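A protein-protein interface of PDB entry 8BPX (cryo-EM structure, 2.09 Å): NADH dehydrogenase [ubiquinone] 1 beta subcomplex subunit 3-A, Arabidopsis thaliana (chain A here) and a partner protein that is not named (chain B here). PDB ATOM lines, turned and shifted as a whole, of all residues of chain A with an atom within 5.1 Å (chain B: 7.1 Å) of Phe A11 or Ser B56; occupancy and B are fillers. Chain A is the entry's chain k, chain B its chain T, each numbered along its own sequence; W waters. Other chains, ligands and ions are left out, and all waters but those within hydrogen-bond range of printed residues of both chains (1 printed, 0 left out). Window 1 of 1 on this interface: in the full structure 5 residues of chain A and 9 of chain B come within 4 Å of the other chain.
Water W1 lies within hydrogen-bond range of the backbone carbonyl oxygen of Ala B88 (2.6 Å) and the guanidinium group of Arg A15 (3.3 Å).
Among the printed residues, pairs that only touch across the chains: Thr A7 with Pro B58 (3.2 Å), Thr A7 with Lys B59 (3.2 Å), Arg A15 with Val B53 (3.3 Å), Phe A11 with Ala B88 (3.5 Å), Phe A11 with Phe B57 (3.5 Å), Arg A15 with Asp B52 (3.6 Å), Arg A14 with Phe B57 (3.6 Å), Phe A11 with Ser B56 (3.6 Å), Phe A11 with Glu B84 (3.6 Å), Phe A11 with Val B53 (3.6 Å) and Phe A11 with Pro B58 (3.8 Å).
The side-chain hydroxyl (OG) of Ser B56 sits at hydrogen-bond distance from the backbone carbonyl oxygen (O) of Asp B52, at 2.8 Å. The backbone carbonyl oxygen of Val B53 lies within hydrogen-bond range of the side-chain hydroxyl of Ser B56, 3.5 Å away. NE of Arg A14 is in salt-bridge range of OE2 of Glu A10 (2.4 Å).
Printed residues of chain A that touch a printed residue of chain B: Thr A7, Thr A8, Phe A11, Arg A14 and Arg A15. Hydrophobic or aromatic side chains of chain A that line the printed part of chain B: Phe A11. Of the 20 printed residues of chain B, 8 touch a printed residue of chain A. Hydrophobic or aromatic side chains of chain B within 4 Å of the printed part of chain A: Val B53, Phe B57, Pro B58 and Ala B88. Among the printed residues, 15 pairs touch across the chains.
The backbone carbonyl oxygen (O) of Ser B56 sits at hydrogen-bond distance from the guanidinium group (NH1) of Arg A14, 2.8 Å away. The side-chain hydroxyl (OG) of Ser B56 sits at hydrogen-bond distance from the guanidinium group (NH1) of Arg A15 (2.8 Å). OG1 of Thr A8 is in hydrogen-bond range of OE2 of Glu B84 (2.8 Å). The guanidinium group of Arg A14 sits close to the backbone nitrogen of Pro B58, 3.4 Å away.
Phe A11 touches just these residues of chain B: Val B53, Ser B56, Phe B57, Pro B58, Glu B84 and Ala B88. Ser B56 touches three residues of chain A. Printed residues of chain A within 4 Å of Lys B59: Thr A7. Of the printed residues of chain A, Val B53 touches Phe A11 (3.6 Å) and Arg A15 (3.3 Å). Of the printed residues of chain B, Arg A15 touches Asp B52 (3.6 Å), Val B53 (3.3 Å) and Ser B56 (2.8 Å). Glu A10 touches none of the printed residues of chain B. The nearest residue of chain B that does not touch Phe A11 is Ile B85 (4.03 Å). The nearest printed residue of chain A that does not touch Ser B56 is Glu A10 (5.6 Å).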
ATOM      1  N   GLY A   6      14.703  29.469  17.890  1.00  0.00           N
ATOM      2  CA  GLY A   6      14.391  28.145  18.462  1.00  0.00           C
ATOM      3  C   GLY A   6      13.346  27.366  17.701  1.00  0.00           C
ATOM      4  O   GLY A   6      12.583  27.973  16.974  1.00  0.00           O
ATOM      5  N   THR A   7      13.339  26.055  17.886  1.00  0.00           N
ATOM      6  CA  THR A   7      12.362  25.228  17.185  1.00  0.00           C
ATOM      7  C   THR A   7      10.934  25.720  17.418  1.00  0.00           C
ATOM      8  O   THR A   7      10.117  25.725  16.492  1.00  0.00           O
ATOM      9  CB  THR A   7      12.533  23.755  17.588  1.00  0.00           C
ATOM     10  OG1 THR A   7      11.867  22.914  16.642  1.00  0.00           O
ATOM     11  CG2 THR A   7      11.999  23.473  18.990  1.00  0.00           C
ATOM     12  N   THR A   8      10.632  26.190  18.628  1.00  0.00           N
ATOM     13  CA  THR A   8       9.280  26.647  18.941  1.00  0.00           C
ATOM     14  C   THR A   8       8.923  27.908  18.157  1.00  0.00           C
ATOM     15  O   THR A   8       7.873  27.975  17.499  1.00  0.00           O
ATOM     16  CB  THR A   8       9.164  26.892  20.446  1.00  0.00           C
ATOM     17  OG1 THR A   8       9.627  25.736  21.149  1.00  0.00           O
ATOM     18  CG2 THR A   8       7.729  27.181  20.842  1.00  0.00           C
ATOM     19  N   GLY A   9       9.794  28.917  18.215  1.00  0.00           N
ATOM     20  CA  GLY A   9       9.546  30.138  17.468  1.00  0.00           C
ATOM     21  C   GLY A   9       9.548  29.913  15.971  1.00  0.00           C
ATOM     22  O   GLY A   9       8.797  30.555  15.238  1.00  0.00           O
ATOM     23  N   GLU A  10      10.395  28.998  15.499  1.00  0.00           N
ATOM     24  CA  GLU A  10      10.432  28.665  14.082  1.00  0.00           C
ATOM     25  C   GLU A  10       9.126  28.027  13.629  1.00  0.00           C
ATOM     26  O   GLU A  10       8.598  28.361  12.562  1.00  0.00           O
ATOM     27  CB  GLU A  10      11.617  27.738  13.811  1.00  0.00           C
ATOM     28  CG  GLU A  10      11.494  26.886  12.562  1.00  0.00           C
ATOM     29  CD  GLU A  10      11.442  27.699  11.291  1.00  0.00           C
ATOM     30  OE1 GLU A  10      11.927  28.852  11.292  1.00  0.00           O
ATOM     31  OE2 GLU A  10      10.919  27.179  10.287  1.00  0.00           O
ATOM     32  N   PHE A  11       8.584  27.113  14.435  1.00  0.00           N
ATOM     33  CA  PHE A  11       7.297  26.508  14.120  1.00  0.00           C
ATOM     34  C   PHE A  11       6.192  27.557  14.088  1.00  0.00           C
ATOM     35  O   PHE A  11       5.363  27.580  13.164  1.00  0.00           O
ATOM     36  CB  PHE A  11       7.003  25.414  15.146  1.00  0.00           C
ATOM     37  CG  PHE A  11       5.624  24.846  15.067  1.00  0.00           C
ATOM     38  CD1 PHE A  11       5.136  24.332  13.881  1.00  0.00           C
ATOM     39  CD2 PHE A  11       4.820  24.805  16.192  1.00  0.00           C
ATOM     40  CE1 PHE A  11       3.867  23.802  13.817  1.00  0.00           C
ATOM     41  CE2 PHE A  11       3.547  24.270  16.132  1.00  0.00           C
ATOM     42  CZ  PHE A  11       3.075  23.769  14.941  1.00  0.00           C
ATOM     43  N   PHE A  12       6.176  28.451  15.076  1.00  0.00           N
ATOM     44  CA  PHE A  12       5.109  29.446  15.114  1.00  0.00           C
ATOM     45  C   PHE A  12       5.244  30.470  13.989  1.00  0.00           C
ATOM     46  O   PHE A  12       4.233  30.945  13.468  1.00  0.00           O
ATOM     47  CB  PHE A  12       5.072  30.115  16.482  1.00  0.00           C
ATOM     48  CG  PHE A  12       4.406  29.277  17.531  1.00  0.00           C
ATOM     49  CD1 PHE A  12       3.118  28.806  17.341  1.00  0.00           C
ATOM     50  CD2 PHE A  12       5.074  28.938  18.696  1.00  0.00           C
ATOM     51  CE1 PHE A  12       2.502  28.023  18.298  1.00  0.00           C
ATOM     52  CE2 PHE A  12       4.461  28.153  19.657  1.00  0.00           C
ATOM     53  CZ  PHE A  12       3.176  27.695  19.459  1.00  0.00           C
ATOM     54  N   ARG A  13       6.470  30.809  13.591  1.00  0.00           N
ATOM     55  CA  ARG A  13       6.656  31.684  12.438  1.00  0.00           C
ATOM     56  C   ARG A  13       6.240  30.993  11.145  1.00  0.00           C
ATOM     57  O   ARG A  13       5.657  31.626  10.257  1.00  0.00           O
ATOM     58  CB  ARG A  13       8.108  32.143  12.348  1.00  0.00           C
ATOM     59  CG  ARG A  13       8.339  33.165  11.261  1.00  0.00           C
ATOM     60  CD  ARG A  13       9.809  33.504  11.119  1.00  0.00           C
ATOM     61  NE  ARG A  13      10.638  32.475  10.489  1.00  0.00           N
ATOM     62  CZ  ARG A  13      10.323  31.724   9.435  1.00  0.00           C
ATOM     63  NH1 ARG A  13       9.199  31.900   8.756  1.00  0.00           N
ATOM     64  NH2 ARG A  13      11.180  30.794   9.026  1.00  0.00           N
ATOM     65  N   ARG A  14       6.528  29.696  11.022  1.00  0.00           N
ATOM     66  CA  ARG A  14       6.086  28.950   9.851  1.00  0.00           C
ATOM     67  C   ARG A  14       4.569  28.947   9.740  1.00  0.00           C
ATOM     68  O   ARG A  14       4.021  29.092   8.643  1.00  0.00           O
ATOM     69  CB  ARG A  14       6.619  27.521   9.908  1.00  0.00           C
ATOM     70  CG  ARG A  14       7.962  27.346   9.251  1.00  0.00           C
ATOM     71  CD  ARG A  14       8.217  25.906   8.884  1.00  0.00           C
ATOM     72  NE  ARG A  14       9.615  25.537   9.065  1.00  0.00           N
ATOM     73  CZ  ARG A  14      10.038  24.312   9.335  1.00  0.00           C
ATOM     74  NH1 ARG A  14       9.194  23.303   9.463  1.00  0.00           N
ATOM     75  NH2 ARG A  14      11.341  24.093   9.473  1.00  0.00           N
ATOM     76  N   ARG A  15       3.870  28.776  10.866  1.00  0.00           N
ATOM     77  CA  ARG A  15       2.412  28.788  10.822  1.00  0.00           C
ATOM     78  C   ARG A  15       1.849  30.157  10.461  1.00  0.00           C
ATOM     79  O   ARG A  15       0.722  30.233   9.962  1.00  0.00           O
ATOM     80  CB  ARG A  15       1.830  28.333  12.162  1.00  0.00           C
ATOM     81  CG  ARG A  15       2.206  26.915  12.565  1.00  0.00           C
ATOM     82  CD  ARG A  15       1.629  25.873  11.630  1.00  0.00           C
ATOM     83  NE  ARG A  15       0.231  26.127  11.309  1.00  0.00           N
ATOM     84  CZ  ARG A  15      -0.324  25.893  10.129  1.00  0.00           C
ATOM     85  NH1 ARG A  15       0.368  25.369   9.131  1.00  0.00           N
ATOM     86  NH2 ARG A  15      -1.607  26.181   9.949  1.00  0.00           N
ATOM     87  N   VAL B  50      -5.594  20.079   9.792  1.00  0.00           N
ATOM     88  CA  VAL B  50      -4.819  19.545  10.906  1.00  0.00           C
ATOM     89  C   VAL B  50      -3.499  18.968  10.413  1.00  0.00           C
ATOM     90  O   VAL B  50      -2.436  19.211  11.000  1.00  0.00           O
ATOM     91  CB  VAL B  50      -5.643  18.499  11.678  1.00  0.00           C
ATOM     92  CG1 VAL B  50      -4.747  17.687  12.596  1.00  0.00           C
ATOM     93  CG2 VAL B  50      -6.756  19.171  12.460  1.00  0.00           C
ATOM     94  N   LEU B  51      -3.542  18.193   9.324  1.00  0.00           N
ATOM     95  CA  LEU B  51      -2.311  17.625   8.792  1.00  0.00           C
ATOM     96  C   LEU B  51      -1.379  18.704   8.260  1.00  0.00           C
ATOM     97  O   LEU B  51      -0.157  18.546   8.317  1.00  0.00           O
ATOM     98  CB  LEU B  51      -2.630  16.595   7.706  1.00  0.00           C
ATOM     99  CG  LEU B  51      -2.466  15.123   8.113  1.00  0.00           C
ATOM    100  CD1 LEU B  51      -3.103  14.840   9.471  1.00  0.00           C
ATOM    101  CD2 LEU B  51      -3.037  14.199   7.058  1.00  0.00           C
ATOM    102  N   ASP B  52      -1.928  19.809   7.745  1.00  0.00           N
ATOM    103  CA  ASP B  52      -1.078  20.931   7.362  1.00  0.00           C
ATOM    104  C   ASP B  52      -0.400  21.549   8.575  1.00  0.00           C
ATOM    105  O   ASP B  52       0.787  21.891   8.524  1.00  0.00           O
ATOM    106  CB  ASP B  52      -1.886  21.985   6.605  1.00  0.00           C
ATOM    107  CG  ASP B  52      -2.466  21.457   5.314  1.00  0.00           C
ATOM    108  OD1 ASP B  52      -1.921  20.473   4.774  1.00  0.00           O
ATOM    109  OD2 ASP B  52      -3.473  22.024   4.839  1.00  0.00           O
ATOM    110  N   VAL B  53      -1.136  21.695   9.682  1.00  0.00           N
ATOM    111  CA  VAL B  53      -0.535  22.232  10.900  1.00  0.00           C
ATOM    112  C   VAL B  53       0.613  21.340  11.361  1.00  0.00           C
ATOM    113  O   VAL B  53       1.713  21.819  11.666  1.00  0.00           O
ATOM    114  CB  VAL B  53      -1.593  22.396  12.006  1.00  0.00           C
ATOM    115  CG1 VAL B  53      -0.919  22.632  13.346  1.00  0.00           C
ATOM    116  CG2 VAL B  53      -2.539  23.540  11.682  1.00  0.00           C
ATOM    117  N   VAL B  54       0.382  20.026  11.394  1.00  0.00           N
ATOM    118  CA  VAL B  54       1.422  19.107  11.856  1.00  0.00           C
ATOM    119  C   VAL B  54       2.603  19.096  10.890  1.00  0.00           C
ATOM    120  O   VAL B  54       3.762  18.974  11.305  1.00  0.00           O
ATOM    121  CB  VAL B  54       0.847  17.695  12.069  1.00  0.00           C
ATOM    122  CG1 VAL B  54       1.875  16.804  12.729  1.00  0.00           C
ATOM    123  CG2 VAL B  54      -0.412  17.756  12.922  1.00  0.00           C
ATOM    124  N   LYS B  55       2.332  19.230   9.590  1.00  0.00           N
ATOM    125  CA  LYS B  55       3.390  19.214   8.590  1.00  0.00           C
ATOM    126  C   LYS B  55       4.371  20.368   8.758  1.00  0.00           C
ATOM    127  O   LYS B  55       5.535  20.237   8.369  1.00  0.00           O
ATOM    128  CB  LYS B  55       2.772  19.260   7.193  1.00  0.00           C
ATOM    129  CG  LYS B  55       2.898  17.978   6.397  1.00  0.00           C
ATOM    130  CD  LYS B  55       1.739  17.841   5.421  1.00  0.00           C
ATOM    131  CE  LYS B  55       1.418  16.397   5.131  1.00  0.00           C
ATOM    132  NZ  LYS B  55       0.693  16.234   3.840  1.00  0.00           N
ATOM    133  N   SER B  56       3.937  21.485   9.341  1.00  0.00           N
ATOM    134  CA  SER B  56       4.798  22.650   9.485  1.00  0.00           C
ATOM    135  C   SER B  56       5.822  22.506  10.602  1.00  0.00           C
ATOM    136  O   SER B  56       6.679  23.383  10.741  1.00  0.00           O
ATOM    137  CB  SER B  56       3.960  23.904   9.744  1.00  0.00           C
ATOM    138  OG  SER B  56       2.738  23.861   9.042  1.00  0.00           O
ATOM    139  N   PHE B  57       5.753  21.448  11.401  1.00  0.00           N
ATOM    140  CA  PHE B  57       6.696  21.312  12.505  1.00  0.00           C
ATOM    141  C   PHE B  57       8.080  20.953  11.979  1.00  0.00           C
ATOM    142  O   PHE B  57       8.206  20.051  11.148  1.00  0.00           O
ATOM    143  CB  PHE B  57       6.224  20.267  13.503  1.00  0.00           C
ATOM    144  CG  PHE B  57       6.774  20.473  14.875  1.00  0.00           C
ATOM    145  CD1 PHE B  57       6.267  21.469  15.689  1.00  0.00           C
ATOM    146  CD2 PHE B  57       7.810  19.690  15.348  1.00  0.00           C
ATOM    147  CE1 PHE B  57       6.777  21.676  16.947  1.00  0.00           C
ATOM    148  CE2 PHE B  57       8.321  19.894  16.609  1.00  0.00           C
ATOM    149  CZ  PHE B  57       7.805  20.886  17.407  1.00  0.00           C
ATOM    150  N   PRO B  58       9.134  21.628  12.447  1.00  0.00           N
ATOM    151  CA  PRO B  58      10.464  21.423  11.840  1.00  0.00           C
ATOM    152  C   PRO B  58      11.027  20.020  12.014  1.00  0.00           C
ATOM    153  O   PRO B  58      11.569  19.460  11.053  1.00  0.00           O
ATOM    154  CB  PRO B  58      11.329  22.484  12.534  1.00  0.00           C
ATOM    155  CG  PRO B  58      10.558  22.931  13.721  1.00  0.00           C
ATOM    156  CD  PRO B  58       9.119  22.738  13.412  1.00  0.00           C
ATOM    157  N   LYS B  59      10.929  19.430  13.209  1.00  0.00           N
ATOM    158  CA  LYS B  59      11.387  18.053  13.369  1.00  0.00           C
ATOM    159  C   LYS B  59      10.568  17.088  12.519  1.00  0.00           C
ATOM    160  O   LYS B  59      11.115  16.144  11.941  1.00  0.00           O
ATOM    161  CB  LYS B  59      11.350  17.628  14.834  1.00  0.00           C
ATOM    162  CG  LYS B  59      11.406  18.727  15.859  1.00  0.00           C
ATOM    163  CD  LYS B  59      12.846  19.032  16.228  1.00  0.00           C
ATOM    164  CE  LYS B  59      12.929  19.948  17.428  1.00  0.00           C
ATOM    165  NZ  LYS B  59      14.198  19.750  18.185  1.00  0.00           N
ATOM    166  N   VAL B  60       9.253  17.300  12.439  1.00  0.00           N
ATOM    167  CA  VAL B  60       8.399  16.401  11.671  1.00  0.00           C
ATOM    168  C   VAL B  60       8.781  16.474  10.201  1.00  0.00           C
ATOM    169  O   VAL B  60       8.863  17.561   9.615  1.00  0.00           O
ATOM    170  CB  VAL B  60       6.920  16.743  11.882  1.00  0.00           C
ATOM    171  CG1 VAL B  60       6.101  16.315  10.684  1.00  0.00           C
ATOM    172  CG2 VAL B  60       6.401  16.080  13.141  1.00  0.00           C
ATOM    173  N   PRO B  62       7.733  16.024   6.445  1.00  0.00           N
ATOM    174  CA  PRO B  62       6.452  15.971   5.735  1.00  0.00           C
ATOM    175  C   PRO B  62       6.369  14.829   4.734  1.00  0.00           C
ATOM    176  O   PRO B  62       6.131  15.054   3.542  1.00  0.00           O
ATOM    177  CB  PRO B  62       6.382  17.335   5.030  1.00  0.00           C
ATOM    178  CG  PRO B  62       7.518  18.147   5.602  1.00  0.00           C
ATOM    179  CD  PRO B  62       8.552  17.159   6.006  1.00  0.00           C
ATOM    180  N   ASP B  81       6.718  19.387  22.346  1.00  0.00           N
ATOM    181  CA  ASP B  81       6.386  19.617  20.946  1.00  0.00           C
ATOM    182  C   ASP B  81       4.912  19.360  20.693  1.00  0.00           C
ATOM    183  O   ASP B  81       4.267  20.084  19.927  1.00  0.00           O
ATOM    184  CB  ASP B  81       7.243  18.725  20.052  1.00  0.00           C
ATOM    185  CG  ASP B  81       8.690  18.684  20.490  1.00  0.00           C
ATOM    186  OD1 ASP B  81       9.158  19.681  21.071  1.00  0.00           O
ATOM    187  OD2 ASP B  81       9.359  17.661  20.250  1.00  0.00           O
ATOM    188  N   VAL B  83       2.531  19.778  22.865  1.00  0.00           N
ATOM    189  CA  VAL B  83       1.831  20.936  23.418  1.00  0.00           C
ATOM    190  C   VAL B  83       1.855  22.096  22.430  1.00  0.00           C
ATOM    191  O   VAL B  83       0.843  22.778  22.220  1.00  0.00           O
ATOM    192  CB  VAL B  83       2.446  21.331  24.775  1.00  0.00           C
ATOM    193  CG1 VAL B  83       1.683  22.481  25.382  1.00  0.00           C
ATOM    194  CG2 VAL B  83       2.451  20.150  25.720  1.00  0.00           C
ATOM    195  N   GLU B  84       3.011  22.335  21.806  1.00  0.00           N
ATOM    196  CA  GLU B  84       3.095  23.383  20.792  1.00  0.00           C
ATOM    197  C   GLU B  84       2.168  23.104  19.610  1.00  0.00           C
ATOM    198  O   GLU B  84       1.495  24.015  19.114  1.00  0.00           O
ATOM    199  CB  GLU B  84       4.539  23.544  20.315  1.00  0.00           C
ATOM    200  CG  GLU B  84       5.461  24.168  21.349  1.00  0.00           C
ATOM    201  CD  GLU B  84       6.896  23.723  21.191  1.00  0.00           C
ATOM    202  OE1 GLU B  84       7.238  23.192  20.116  1.00  0.00           O
ATOM    203  OE2 GLU B  84       7.687  23.910  22.136  1.00  0.00           O
ATOM    204  N   ILE B  85       2.122  21.854  19.143  1.00  0.00           N
ATOM    205  CA  ILE B  85       1.271  21.515  18.003  1.00  0.00           C
ATOM    206  C   ILE B  85      -0.202  21.684  18.363  1.00  0.00           C
ATOM    207  O   ILE B  85      -1.010  22.141  17.543  1.00  0.00           O
ATOM    208  CB  ILE B  85       1.579  20.090  17.502  1.00  0.00           C
ATOM    209  CG1 ILE B  85       2.850  20.073  16.652  1.00  0.00           C
ATOM    210  CG2 ILE B  85       0.420  19.535  16.687  1.00  0.00           C
ATOM    211  CD1 ILE B  85       3.762  18.896  16.921  1.00  0.00           C
ATOM    212  N   VAL B  86      -0.578  21.322  19.590  1.00  0.00           N
ATOM    213  CA  VAL B  86      -1.959  21.507  20.024  1.00  0.00           C
ATOM    214  C   VAL B  86      -2.304  22.991  20.084  1.00  0.00           C
ATOM    215  O   VAL B  86      -3.393  23.400  19.672  1.00  0.00           O
ATOM    216  CB  VAL B  86      -2.200  20.801  21.371  1.00  0.00           C
ATOM    217  CG1 VAL B  86      -3.547  21.198  21.957  1.00  0.00           C
ATOM    218  CG2 VAL B  86      -2.125  19.295  21.193  1.00  0.00           C
ATOM    219  N   MET B  87      -1.394  23.837  20.604  1.00  0.00           N
ATOM    220  CA  MET B  87      -1.590  25.316  20.589  1.00  0.00           C
ATOM    221  C   MET B  87      -1.731  25.820  19.136  1.00  0.00           C
ATOM    222  O   MET B  87      -2.564  26.652  18.911  1.00  0.00           O
ATOM    223  CB  MET B  87      -0.497  26.092  21.342  1.00  0.00           C
ATOM    224  CG  MET B  87      -0.702  27.609  21.351  1.00  0.00           C
ATOM    225  SD  MET B  87       0.420  28.634  22.360  1.00  0.00           S
ATOM    226  CE  MET B  87      -0.110  30.284  21.904  1.00  0.00           C
ATOM    227  N   ALA B  88      -0.979  25.250  18.207  1.00  0.00           N
ATOM    228  CA  ALA B  88      -1.088  25.677  16.814  1.00  0.00           C
ATOM    229  C   ALA B  88      -2.434  25.283  16.213  1.00  0.00           C
ATOM    230  O   ALA B  88      -3.028  26.052  15.454  1.00  0.00           O
ATOM    231  CB  ALA B  88       0.058  25.097  15.993  1.00  0.00           C
ATOM    232  N   ILE B  89      -2.928  24.087  16.540  1.00  0.00           N
ATOM    233  CA  ILE B  89      -4.260  23.673  16.095  1.00  0.00           C
ATOM    234  C   ILE B  89      -5.325  24.590  16.691  1.00  0.00           C
ATOM    235  O   ILE B  89      -6.286  24.992  16.014  1.00  0.00           O
ATOM    236  CB  ILE B  89      -4.504  22.197  16.462  1.00  0.00           C
ATOM    237  CG1 ILE B  89      -3.687  21.277  15.555  1.00  0.00           C
ATOM    238  CG2 ILE B  89      -5.983  21.845  16.378  1.00  0.00           C
ATOM    239  CD1 ILE B  89      -3.402  19.914  16.158  1.00  0.00           C
HETATM  240  O   HOH W   1      -1.777  27.343  13.570  1.00  0.00           O
